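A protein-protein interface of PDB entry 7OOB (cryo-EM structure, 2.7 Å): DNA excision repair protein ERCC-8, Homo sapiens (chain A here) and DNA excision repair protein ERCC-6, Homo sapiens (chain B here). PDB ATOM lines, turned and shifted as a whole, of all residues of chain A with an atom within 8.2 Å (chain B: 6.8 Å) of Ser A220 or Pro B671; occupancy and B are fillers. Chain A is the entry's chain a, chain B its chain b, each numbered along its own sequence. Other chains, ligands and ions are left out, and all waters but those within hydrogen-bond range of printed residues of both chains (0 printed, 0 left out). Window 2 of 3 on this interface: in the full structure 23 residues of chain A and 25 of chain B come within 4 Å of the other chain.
Hydrophobic or aromatic side chains of chain A that line the printed part of chain B: Ala A219.
Of the 20 printed residues of chain B, 6 touch a printed residue of chain A.
Among the printed residues, no Asp or Glu carboxylate lies within 4 Å of a Lys or Arg side-chain nitrogen of the other chain.
N of Gly B530 lies within hydrogen-bond range of O of Ile B695 (3.4 Å).
The guanidinium group (NE) of Arg B673 lies close to the backbone carbonyl oxygen (O) of Thr B670 (3.1 Å).
O of Pro B671 is in hydrogen-bond range of NE of Arg B673 (3.0 Å).
The guanidinium group (NH2) of Arg B673 sits at hydrogen-bond distance from the backbone carbonyl oxygen (O) of Ile B695, at 3.1 Å.
The side-chain carboxylate (OD1) of Asp A215 lies within salt-bridge range of the guanidinium group (NE) of Arg A217, 3.6 Å away.
The guanidinium group (NH2) of Arg A218 is in salt-bridge range of the side-chain carboxylate (OD2) of Asp A215 (3.4 Å).
The side-chain amide oxygen of Gln B528 sits close to the guanidinium group of Arg A218, at 3.0 Å.
O of Gln B528 lies within hydrogen-bond range of N of Ala A219 (3.2 Å).
The guanidinium group of Arg B673 sits at hydrogen-bond distance from the backbone carbonyl oxygen of Ala A219 (3.2 Å).
Printed residues of chain B within 4 Å of Ala A219: Gln B528, Arg B673, Ile B695 and Phe B696.
Printed residues of chain B within 4 Å of Ser A220: Pro B671.
Gly A221 touches none of the printed residues of chain B.
Of the printed residues of chain A, Gln B528 touches Arg A218 and Ala A219.
His B672 touches none of the printed residues of chain A.
Of the printed residues of chain A, Arg B673 touches Ala A219.
The nearest residue of chain A that does not touch Pro B671 is Ala A219 (4.2 Å).
The nearest printed residue of chain A that does not touch Phe B696 is Val A216 (4.03 Å).
O of Arg A217 touches O of Gln B527 (3.7 Å).
Arg A217 touches Phe B696 (O to CE1, 3.7 Å).
Arg A218 touches Gln B527 (CA to O, 3.9 Å).
Arg A218 touches Phe B696.
Ala A219 touches Ile B695 (CB to O, 3.96 Å).
CB of Ala A219 touches CD1 of Phe B696, 3.3 Å away.
CB of Ser A220 touches CB of Pro B671 (3.98 Å).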
ATOM      1  N   GLN A 183       0.778  13.381   8.829  1.00  0.00           N
ATOM      2  CA  GLN A 183       2.199  13.685   8.870  1.00  0.00           C
ATOM      3  C   GLN A 183       2.538  14.402  10.169  1.00  0.00           C
ATOM      4  O   GLN A 183       1.739  15.178  10.698  1.00  0.00           O
ATOM      5  CB  GLN A 183       2.614  14.530   7.662  1.00  0.00           C
ATOM      6  CG  GLN A 183       1.998  15.913   7.601  1.00  0.00           C
ATOM      7  CD  GLN A 183       2.404  16.660   6.349  1.00  0.00           C
ATOM      8  OE1 GLN A 183       3.191  16.162   5.544  1.00  0.00           O
ATOM      9  NE2 GLN A 183       1.878  17.867   6.183  1.00  0.00           N
ATOM     10  N   TRP A 214      -4.224  11.312  17.189  1.00  0.00           N
ATOM     11  CA  TRP A 214      -4.769  12.091  16.094  1.00  0.00           C
ATOM     12  C   TRP A 214      -6.284  12.035  16.146  1.00  0.00           C
ATOM     13  O   TRP A 214      -6.869  11.086  16.672  1.00  0.00           O
ATOM     14  CB  TRP A 214      -4.328  11.548  14.730  1.00  0.00           C
ATOM     15  CG  TRP A 214      -2.875  11.304  14.580  1.00  0.00           C
ATOM     16  CD1 TRP A 214      -2.168  10.245  15.059  1.00  0.00           C
ATOM     17  CD2 TRP A 214      -1.943  12.128  13.881  1.00  0.00           C
ATOM     18  NE1 TRP A 214      -0.848  10.360  14.707  1.00  0.00           N
ATOM     19  CE2 TRP A 214      -0.684  11.510  13.983  1.00  0.00           C
ATOM     20  CE3 TRP A 214      -2.049  13.331  13.180  1.00  0.00           C
ATOM     21  CZ2 TRP A 214       0.460  12.054  13.413  1.00  0.00           C
ATOM     22  CZ3 TRP A 214      -0.914  13.869  12.616  1.00  0.00           C
ATOM     23  CH2 TRP A 214       0.324  13.232  12.735  1.00  0.00           C
ATOM     24  N   ASP A 215      -6.905  13.040  15.537  1.00  0.00           N
ATOM     25  CA  ASP A 215      -8.336  13.071  15.250  1.00  0.00           C
ATOM     26  C   ASP A 215      -8.428  13.172  13.732  1.00  0.00           C
ATOM     27  O   ASP A 215      -8.362  14.268  13.172  1.00  0.00           O
ATOM     28  CB  ASP A 215      -9.022  14.240  15.946  1.00  0.00           C
ATOM     29  CG  ASP A 215     -10.523  14.275  15.710  1.00  0.00           C
ATOM     30  OD1 ASP A 215     -11.029  13.536  14.842  1.00  0.00           O
ATOM     31  OD2 ASP A 215     -11.206  15.056  16.404  1.00  0.00           O
ATOM     32  N   VAL A 216      -8.580  12.024  13.066  1.00  0.00           N
ATOM     33  CA  VAL A 216      -8.456  11.975  11.613  1.00  0.00           C
ATOM     34  C   VAL A 216      -9.461  12.885  10.911  1.00  0.00           C
ATOM     35  O   VAL A 216      -9.257  13.239   9.746  1.00  0.00           O
ATOM     36  CB  VAL A 216      -8.574  10.515  11.115  1.00  0.00           C
ATOM     37  CG1 VAL A 216      -7.497   9.644  11.753  1.00  0.00           C
ATOM     38  CG2 VAL A 216      -9.951   9.940  11.406  1.00  0.00           C
ATOM     39  N   ARG A 217     -10.542  13.275  11.587  1.00  0.00           N
ATOM     40  CA  ARG A 217     -11.409  14.322  11.053  1.00  0.00           C
ATOM     41  C   ARG A 217     -10.690  15.659  11.010  1.00  0.00           C
ATOM     42  O   ARG A 217     -10.870  16.441  10.071  1.00  0.00           O
ATOM     43  CB  ARG A 217     -12.657  14.465  11.913  1.00  0.00           C
ATOM     44  CG  ARG A 217     -13.690  13.394  11.712  1.00  0.00           C
ATOM     45  CD  ARG A 217     -14.883  13.605  12.628  1.00  0.00           C
ATOM     46  NE  ARG A 217     -14.477  13.770  14.021  1.00  0.00           N
ATOM     47  CZ  ARG A 217     -15.246  14.266  14.984  1.00  0.00           C
ATOM     48  NH1 ARG A 217     -16.488  14.661  14.730  1.00  0.00           N
ATOM     49  NH2 ARG A 217     -14.765  14.373  16.215  1.00  0.00           N
ATOM     50  N   ARG A 218      -9.891  15.940  12.030  1.00  0.00           N
ATOM     51  CA  ARG A 218      -9.296  17.252  12.198  1.00  0.00           C
ATOM     52  C   ARG A 218      -8.318  17.572  11.076  1.00  0.00           C
ATOM     53  O   ARG A 218      -7.682  16.687  10.499  1.00  0.00           O
ATOM     54  CB  ARG A 218      -8.583  17.329  13.542  1.00  0.00           C
ATOM     55  CG  ARG A 218      -8.228  18.747  13.948  1.00  0.00           C
ATOM     56  CD  ARG A 218      -8.090  18.960  15.454  1.00  0.00           C
ATOM     57  NE  ARG A 218      -9.168  18.356  16.232  1.00  0.00           N
ATOM     58  CZ  ARG A 218      -9.267  18.421  17.555  1.00  0.00           C
ATOM     59  NH1 ARG A 218      -8.364  19.080  18.271  1.00  0.00           N
ATOM     60  NH2 ARG A 218     -10.285  17.834  18.166  1.00  0.00           N
ATOM     61  N   ALA A 219      -8.191  18.866  10.788  1.00  0.00           N
ATOM     62  CA  ALA A 219      -7.325  19.380   9.737  1.00  0.00           C
ATOM     63  C   ALA A 219      -6.118  20.116  10.302  1.00  0.00           C
ATOM     64  O   ALA A 219      -5.548  20.980   9.633  1.00  0.00           O
ATOM     65  CB  ALA A 219      -8.109  20.329   8.833  1.00  0.00           C
ATOM     66  N   SER A 220      -5.717  19.792  11.534  1.00  0.00           N
ATOM     67  CA  SER A 220      -4.732  20.603  12.240  1.00  0.00           C
ATOM     68  C   SER A 220      -3.748  19.758  13.041  1.00  0.00           C
ATOM     69  O   SER A 220      -3.289  20.183  14.106  1.00  0.00           O
ATOM     70  CB  SER A 220      -5.425  21.614  13.156  1.00  0.00           C
ATOM     71  OG  SER A 220      -6.221  20.969  14.132  1.00  0.00           O
ATOM     72  N   GLY A 221      -3.417  18.569  12.557  1.00  0.00           N
ATOM     73  CA  GLY A 221      -2.335  17.813  13.147  1.00  0.00           C
ATOM     74  C   GLY A 221      -2.747  17.015  14.369  1.00  0.00           C
ATOM     75  O   GLY A 221      -3.916  16.940  14.754  1.00  0.00           O
ATOM     76  N   CYS A 222      -1.739  16.409  14.992  1.00  0.00           N
ATOM     77  CA  CYS A 222      -1.983  15.480  16.084  1.00  0.00           C
ATOM     78  C   CYS A 222      -2.561  16.205  17.291  1.00  0.00           C
ATOM     79  O   CYS A 222      -2.194  17.342  17.594  1.00  0.00           O
ATOM     80  CB  CYS A 222      -0.690  14.755  16.465  1.00  0.00           C
ATOM     81  SG  CYS A 222       0.567  15.742  17.323  1.00  0.00           S
ATOM     82  N   LEU A 223      -3.502  15.543  17.963  1.00  0.00           N
ATOM     83  CA  LEU A 223      -4.050  16.091  19.198  1.00  0.00           C
ATOM     84  C   LEU A 223      -2.977  16.209  20.269  1.00  0.00           C
ATOM     85  O   LEU A 223      -2.783  17.278  20.860  1.00  0.00           O
ATOM     86  CB  LEU A 223      -5.180  15.199  19.704  1.00  0.00           C
ATOM     87  CG  LEU A 223      -6.564  15.338  19.091  1.00  0.00           C
ATOM     88  CD1 LEU A 223      -7.363  14.093  19.392  1.00  0.00           C
ATOM     89  CD2 LEU A 223      -7.253  16.556  19.650  1.00  0.00           C
ATOM     90  N   LEU B 524     -18.682  21.452   9.058  1.00  0.00           N
ATOM     91  CA  LEU B 524     -17.240  21.639   8.892  1.00  0.00           C
ATOM     92  C   LEU B 524     -16.608  22.183  10.160  1.00  0.00           C
ATOM     93  O   LEU B 524     -15.538  21.728  10.578  1.00  0.00           O
ATOM     94  CB  LEU B 524     -16.968  22.589   7.739  1.00  0.00           C
ATOM     95  CG  LEU B 524     -16.560  21.938   6.432  1.00  0.00           C
ATOM     96  CD1 LEU B 524     -17.555  20.908   5.949  1.00  0.00           C
ATOM     97  CD2 LEU B 524     -16.442  23.029   5.433  1.00  0.00           C
ATOM     98  N   GLN B 527     -16.429  19.347  12.837  1.00  0.00           N
ATOM     99  CA  GLN B 527     -15.351  18.403  12.574  1.00  0.00           C
ATOM    100  C   GLN B 527     -13.989  19.077  12.515  1.00  0.00           C
ATOM    101  O   GLN B 527     -12.981  18.382  12.361  1.00  0.00           O
ATOM    102  CB  GLN B 527     -15.596  17.662  11.258  1.00  0.00           C
ATOM    103  CG  GLN B 527     -16.972  17.029  11.128  1.00  0.00           C
ATOM    104  CD  GLN B 527     -17.331  16.722   9.696  1.00  0.00           C
ATOM    105  OE1 GLN B 527     -16.517  16.886   8.791  1.00  0.00           O
ATOM    106  NE2 GLN B 527     -18.567  16.298   9.479  1.00  0.00           N
ATOM    107  N   GLN B 528     -13.940  20.403  12.635  1.00  0.00           N
ATOM    108  CA  GLN B 528     -12.691  21.159  12.607  1.00  0.00           C
ATOM    109  C   GLN B 528     -11.952  20.941  11.292  1.00  0.00           C
ATOM    110  O   GLN B 528     -10.727  20.836  11.252  1.00  0.00           O
ATOM    111  CB  GLN B 528     -11.809  20.805  13.802  1.00  0.00           C
ATOM    112  CG  GLN B 528     -12.345  21.352  15.096  1.00  0.00           C
ATOM    113  CD  GLN B 528     -11.331  21.308  16.203  1.00  0.00           C
ATOM    114  OE1 GLN B 528     -11.328  20.391  17.018  1.00  0.00           O
ATOM    115  NE2 GLN B 528     -10.451  22.298  16.236  1.00  0.00           N
ATOM    116  N   ALA B 529     -12.714  20.877  10.208  1.00  0.00           N
ATOM    117  CA  ALA B 529     -12.186  20.775   8.862  1.00  0.00           C
ATOM    118  C   ALA B 529     -12.459  22.068   8.114  1.00  0.00           C
ATOM    119  O   ALA B 529     -13.295  22.882   8.516  1.00  0.00           O
ATOM    120  CB  ALA B 529     -12.811  19.598   8.108  1.00  0.00           C
ATOM    121  N   GLY B 530     -11.726  22.253   7.024  1.00  0.00           N
ATOM    122  CA  GLY B 530     -12.017  23.295   6.073  1.00  0.00           C
ATOM    123  C   GLY B 530     -12.802  22.753   4.894  1.00  0.00           C
ATOM    124  O   GLY B 530     -12.971  21.550   4.725  1.00  0.00           O
ATOM    125  N   GLY B 531     -13.284  23.671   4.066  1.00  0.00           N
ATOM    126  CA  GLY B 531     -14.021  23.261   2.887  1.00  0.00           C
ATOM    127  C   GLY B 531     -14.092  24.357   1.855  1.00  0.00           C
ATOM    128  O   GLY B 531     -13.675  25.495   2.079  1.00  0.00           O
ATOM    129  N   ARG B 565     -11.767  27.948  23.535  1.00  0.00           N
ATOM    130  CA  ARG B 565     -10.769  28.976  23.259  1.00  0.00           C
ATOM    131  C   ARG B 565     -11.462  30.309  22.943  1.00  0.00           C
ATOM    132  O   ARG B 565     -11.561  31.175  23.813  1.00  0.00           O
ATOM    133  CB  ARG B 565      -9.850  28.522  22.119  1.00  0.00           C
ATOM    134  CG  ARG B 565      -8.526  29.256  22.035  1.00  0.00           C
ATOM    135  CD  ARG B 565      -7.711  28.722  20.868  1.00  0.00           C
ATOM    136  NE  ARG B 565      -6.425  29.394  20.715  1.00  0.00           N
ATOM    137  CZ  ARG B 565      -5.452  28.981  19.906  1.00  0.00           C
ATOM    138  NH1 ARG B 565      -5.604  27.892  19.159  1.00  0.00           N
ATOM    139  NH2 ARG B 565      -4.317  29.662  19.839  1.00  0.00           N
ATOM    140  N   TRP B 643      -5.826  33.391  14.177  1.00  0.00           N
ATOM    141  CA  TRP B 643      -7.122  33.741  13.621  1.00  0.00           C
ATOM    142  C   TRP B 643      -8.064  32.551  13.724  1.00  0.00           C
ATOM    143  O   TRP B 643      -7.633  31.398  13.790  1.00  0.00           O
ATOM    144  CB  TRP B 643      -6.960  34.189  12.169  1.00  0.00           C
ATOM    145  CG  TRP B 643      -5.948  35.266  12.055  1.00  0.00           C
ATOM    146  CD1 TRP B 643      -4.607  35.110  11.892  1.00  0.00           C
ATOM    147  CD2 TRP B 643      -6.183  36.670  12.131  1.00  0.00           C
ATOM    148  NE1 TRP B 643      -3.991  36.329  11.861  1.00  0.00           N
ATOM    149  CE2 TRP B 643      -4.938  37.307  12.002  1.00  0.00           C
ATOM    150  CE3 TRP B 643      -7.325  37.454  12.289  1.00  0.00           C
ATOM    151  CZ2 TRP B 643      -4.802  38.686  12.023  1.00  0.00           C
ATOM    152  CZ3 TRP B 643      -7.190  38.824  12.311  1.00  0.00           C
ATOM    153  CH2 TRP B 643      -5.938  39.428  12.180  1.00  0.00           C
ATOM    154  N   HIS B 644      -9.363  32.838  13.765  1.00  0.00           N
ATOM    155  CA  HIS B 644     -10.342  31.778  13.964  1.00  0.00           C
ATOM    156  C   HIS B 644     -10.864  31.214  12.649  1.00  0.00           C
ATOM    157  O   HIS B 644     -11.156  30.018  12.571  1.00  0.00           O
ATOM    158  CB  HIS B 644     -11.505  32.284  14.816  1.00  0.00           C
ATOM    159  CG  HIS B 644     -12.419  31.196  15.284  1.00  0.00           C
ATOM    160  ND1 HIS B 644     -13.737  31.419  15.617  1.00  0.00           N
ATOM    161  CD2 HIS B 644     -12.205  29.873  15.473  1.00  0.00           C
ATOM    162  CE1 HIS B 644     -14.295  30.282  15.993  1.00  0.00           C
ATOM    163  NE2 HIS B 644     -13.386  29.328  15.914  1.00  0.00           N
ATOM    164  N   PHE B 668      -1.491  29.735   7.987  1.00  0.00           N
ATOM    165  CA  PHE B 668      -2.414  29.936   9.091  1.00  0.00           C
ATOM    166  C   PHE B 668      -2.581  28.625   9.844  1.00  0.00           C
ATOM    167  O   PHE B 668      -2.898  27.591   9.247  1.00  0.00           O
ATOM    168  CB  PHE B 668      -3.761  30.434   8.578  1.00  0.00           C
ATOM    169  CG  PHE B 668      -3.720  31.819   8.019  1.00  0.00           C
ATOM    170  CD1 PHE B 668      -3.933  32.914   8.830  1.00  0.00           C
ATOM    171  CD2 PHE B 668      -3.472  32.027   6.678  1.00  0.00           C
ATOM    172  CE1 PHE B 668      -3.901  34.184   8.314  1.00  0.00           C
ATOM    173  CE2 PHE B 668      -3.443  33.298   6.156  1.00  0.00           C
ATOM    174  CZ  PHE B 668      -3.655  34.377   6.974  1.00  0.00           C
ATOM    175  N   ARG B 669      -2.366  28.670  11.156  1.00  0.00           N
ATOM    176  CA  ARG B 669      -2.402  27.467  11.976  1.00  0.00           C
ATOM    177  C   ARG B 669      -3.811  26.932  12.185  1.00  0.00           C
ATOM    178  O   ARG B 669      -3.961  25.770  12.575  1.00  0.00           O
ATOM    179  CB  ARG B 669      -1.740  27.762  13.329  1.00  0.00           C
ATOM    180  CG  ARG B 669      -1.591  26.561  14.259  1.00  0.00           C
ATOM    181  CD  ARG B 669      -2.745  26.449  15.263  1.00  0.00           C
ATOM    182  NE  ARG B 669      -2.561  25.343  16.196  1.00  0.00           N
ATOM    183  CZ  ARG B 669      -3.507  24.873  17.006  1.00  0.00           C
ATOM    184  NH1 ARG B 669      -3.234  23.862  17.819  1.00  0.00           N
ATOM    185  NH2 ARG B 669      -4.731  25.392  16.999  1.00  0.00           N
ATOM    186  N   THR B 670      -4.823  27.700  11.860  1.00  0.00           N
ATOM    187  CA  THR B 670      -6.188  27.411  12.246  1.00  0.00           C
ATOM    188  C   THR B 670      -6.711  26.210  11.444  1.00  0.00           C
ATOM    189  O   THR B 670      -6.205  25.921  10.360  1.00  0.00           O
ATOM    190  CB  THR B 670      -7.033  28.651  11.995  1.00  0.00           C
ATOM    191  OG1 THR B 670      -6.505  29.744  12.754  1.00  0.00           O
ATOM    192  CG2 THR B 670      -8.433  28.465  12.447  1.00  0.00           C
ATOM    193  N   PRO B 671      -7.669  25.441  11.984  1.00  0.00           N
ATOM    194  CA  PRO B 671      -8.297  24.383  11.168  1.00  0.00           C
ATOM    195  C   PRO B 671      -9.420  24.865  10.271  1.00  0.00           C
ATOM    196  O   PRO B 671      -9.675  24.241   9.235  1.00  0.00           O
ATOM    197  CB  PRO B 671      -8.850  23.410  12.216  1.00  0.00           C
ATOM    198  CG  PRO B 671      -9.031  24.227  13.431  1.00  0.00           C
ATOM    199  CD  PRO B 671      -7.921  25.223  13.421  1.00  0.00           C
ATOM    200  N   HIS B 672     -10.100  25.939  10.652  1.00  0.00           N
ATOM    201  CA  HIS B 672     -11.275  26.459   9.960  1.00  0.00           C
ATOM    202  C   HIS B 672     -10.856  27.344   8.784  1.00  0.00           C
ATOM    203  O   HIS B 672     -10.941  28.571   8.806  1.00  0.00           O
ATOM    204  CB  HIS B 672     -12.133  27.225  10.952  1.00  0.00           C
ATOM    205  CG  HIS B 672     -12.448  26.446  12.186  1.00  0.00           C
ATOM    206  ND1 HIS B 672     -13.219  25.306  12.174  1.00  0.00           N
ATOM    207  CD2 HIS B 672     -12.056  26.623  13.470  1.00  0.00           C
ATOM    208  CE1 HIS B 672     -13.312  24.827  13.402  1.00  0.00           C
ATOM    209  NE2 HIS B 672     -12.613  25.607  14.207  1.00  0.00           N
ATOM    210  N   ARG B 673     -10.399  26.676   7.737  1.00  0.00           N
ATOM    211  CA  ARG B 673     -10.078  27.292   6.458  1.00  0.00           C
ATOM    212  C   ARG B 673     -11.252  27.134   5.510  1.00  0.00           C
ATOM    213  O   ARG B 673     -11.764  26.028   5.342  1.00  0.00           O
ATOM    214  CB  ARG B 673      -8.843  26.635   5.854  1.00  0.00           C
ATOM    215  CG  ARG B 673      -7.531  27.073   6.456  1.00  0.00           C
ATOM    216  CD  ARG B 673      -7.244  26.362   7.739  1.00  0.00           C
ATOM    217  NE  ARG B 673      -7.215  24.912   7.628  1.00  0.00           N
ATOM    218  CZ  ARG B 673      -6.168  24.199   7.257  1.00  0.00           C
ATOM    219  NH1 ARG B 673      -5.012  24.769   6.925  1.00  0.00           N
ATOM    220  NH2 ARG B 673      -6.294  22.895   7.212  1.00  0.00           N
ATOM    221  N   ILE B 674     -11.662  28.226   4.877  1.00  0.00           N
ATOM    222  CA  ILE B 674     -12.738  28.189   3.898  1.00  0.00           C
ATOM    223  C   ILE B 674     -12.243  28.820   2.610  1.00  0.00           C
ATOM    224  O   ILE B 674     -11.461  29.777   2.631  1.00  0.00           O
ATOM    225  CB  ILE B 674     -14.013  28.898   4.400  1.00  0.00           C
ATOM    226  CG1 ILE B 674     -14.419  28.399   5.794  1.00  0.00           C
ATOM    227  CG2 ILE B 674     -15.145  28.684   3.414  1.00  0.00           C
ATOM    228  CD1 ILE B 674     -14.838  26.937   5.863  1.00  0.00           C
ATOM    229  N   PHE B 694      -4.940  23.439   0.981  1.00  0.00           N
ATOM    230  CA  PHE B 694      -5.166  24.555   1.890  1.00  0.00           C
ATOM    231  C   PHE B 694      -6.269  24.246   2.900  1.00  0.00           C
ATOM    232  O   PHE B 694      -6.081  24.452   4.102  1.00  0.00           O
ATOM    233  CB  PHE B 694      -5.516  25.825   1.114  1.00  0.00           C
ATOM    234  CG  PHE B 694      -6.063  26.925   1.975  1.00  0.00           C
ATOM    235  CD1 PHE B 694      -5.223  27.693   2.757  1.00  0.00           C
ATOM    236  CD2 PHE B 694      -7.415  27.198   1.996  1.00  0.00           C
ATOM    237  CE1 PHE B 694      -5.726  28.702   3.544  1.00  0.00           C
ATOM    238  CE2 PHE B 694      -7.916  28.209   2.772  1.00  0.00           C
ATOM    239  CZ  PHE B 694      -7.074  28.955   3.554  1.00  0.00           C
ATOM    240  N   ILE B 695      -7.416  23.736   2.445  1.00  0.00           N
ATOM    241  CA  ILE B 695      -8.504  23.513   3.402  1.00  0.00           C
ATOM    242  C   ILE B 695      -8.258  22.297   4.287  1.00  0.00           C
ATOM    243  O   ILE B 695      -8.711  22.265   5.436  1.00  0.00           O
ATOM    244  CB  ILE B 695      -9.869  23.399   2.705  1.00  0.00           C
ATOM    245  CG1 ILE B 695      -9.875  22.292   1.653  1.00  0.00           C
ATOM    246  CG2 ILE B 695     -10.248  24.728   2.101  1.00  0.00           C
ATOM    247  CD1 ILE B 695     -11.225  21.741   1.402  1.00  0.00           C
ATOM    248  N   PHE B 696      -7.586  21.264   3.779  1.00  0.00           N
ATOM    249  CA  PHE B 696      -7.331  20.058   4.562  1.00  0.00           C
ATOM    250  C   PHE B 696      -6.073  19.395   3.993  1.00  0.00           C
ATOM    251  O   PHE B 696      -6.145  18.619   3.030  1.00  0.00           O
ATOM    252  CB  PHE B 696      -8.516  19.101   4.515  1.00  0.00           C
ATOM    253  CG  PHE B 696      -8.332  17.880   5.348  1.00  0.00           C
ATOM    254  CD1 PHE B 696      -8.475  17.891   6.707  1.00  0.00           C
ATOM    255  CD2 PHE B 696      -7.847  16.772   4.775  1.00  0.00           C
ATOM    256  CE1 PHE B 696      -8.263  16.743   7.442  1.00  0.00           C
ATOM    257  CE2 PHE B 696      -7.628  15.624   5.478  1.00  0.00           C
ATOM    258  CZ  PHE B 696      -7.825  15.611   6.817  1.00  0.00           C
ATOM    259  N   PRO B 697      -4.895  19.679   4.570  1.00  0.00           N
ATOM    260  CA  PRO B 697      -3.626  19.298   3.930  1.00  0.00           C
ATOM    261  C   PRO B 697      -3.476  17.834   3.566  1.00  0.00           C
ATOM    262  O   PRO B 697      -2.844  17.531   2.547  1.00  0.00           O
ATOM    263  CB  PRO B 697      -2.600  19.717   4.989  1.00  0.00           C
ATOM    264  CG  PRO B 697      -3.194  20.905   5.587  1.00  0.00           C
ATOM    265  CD  PRO B 697      -4.659  20.664   5.628  1.00  0.00           C
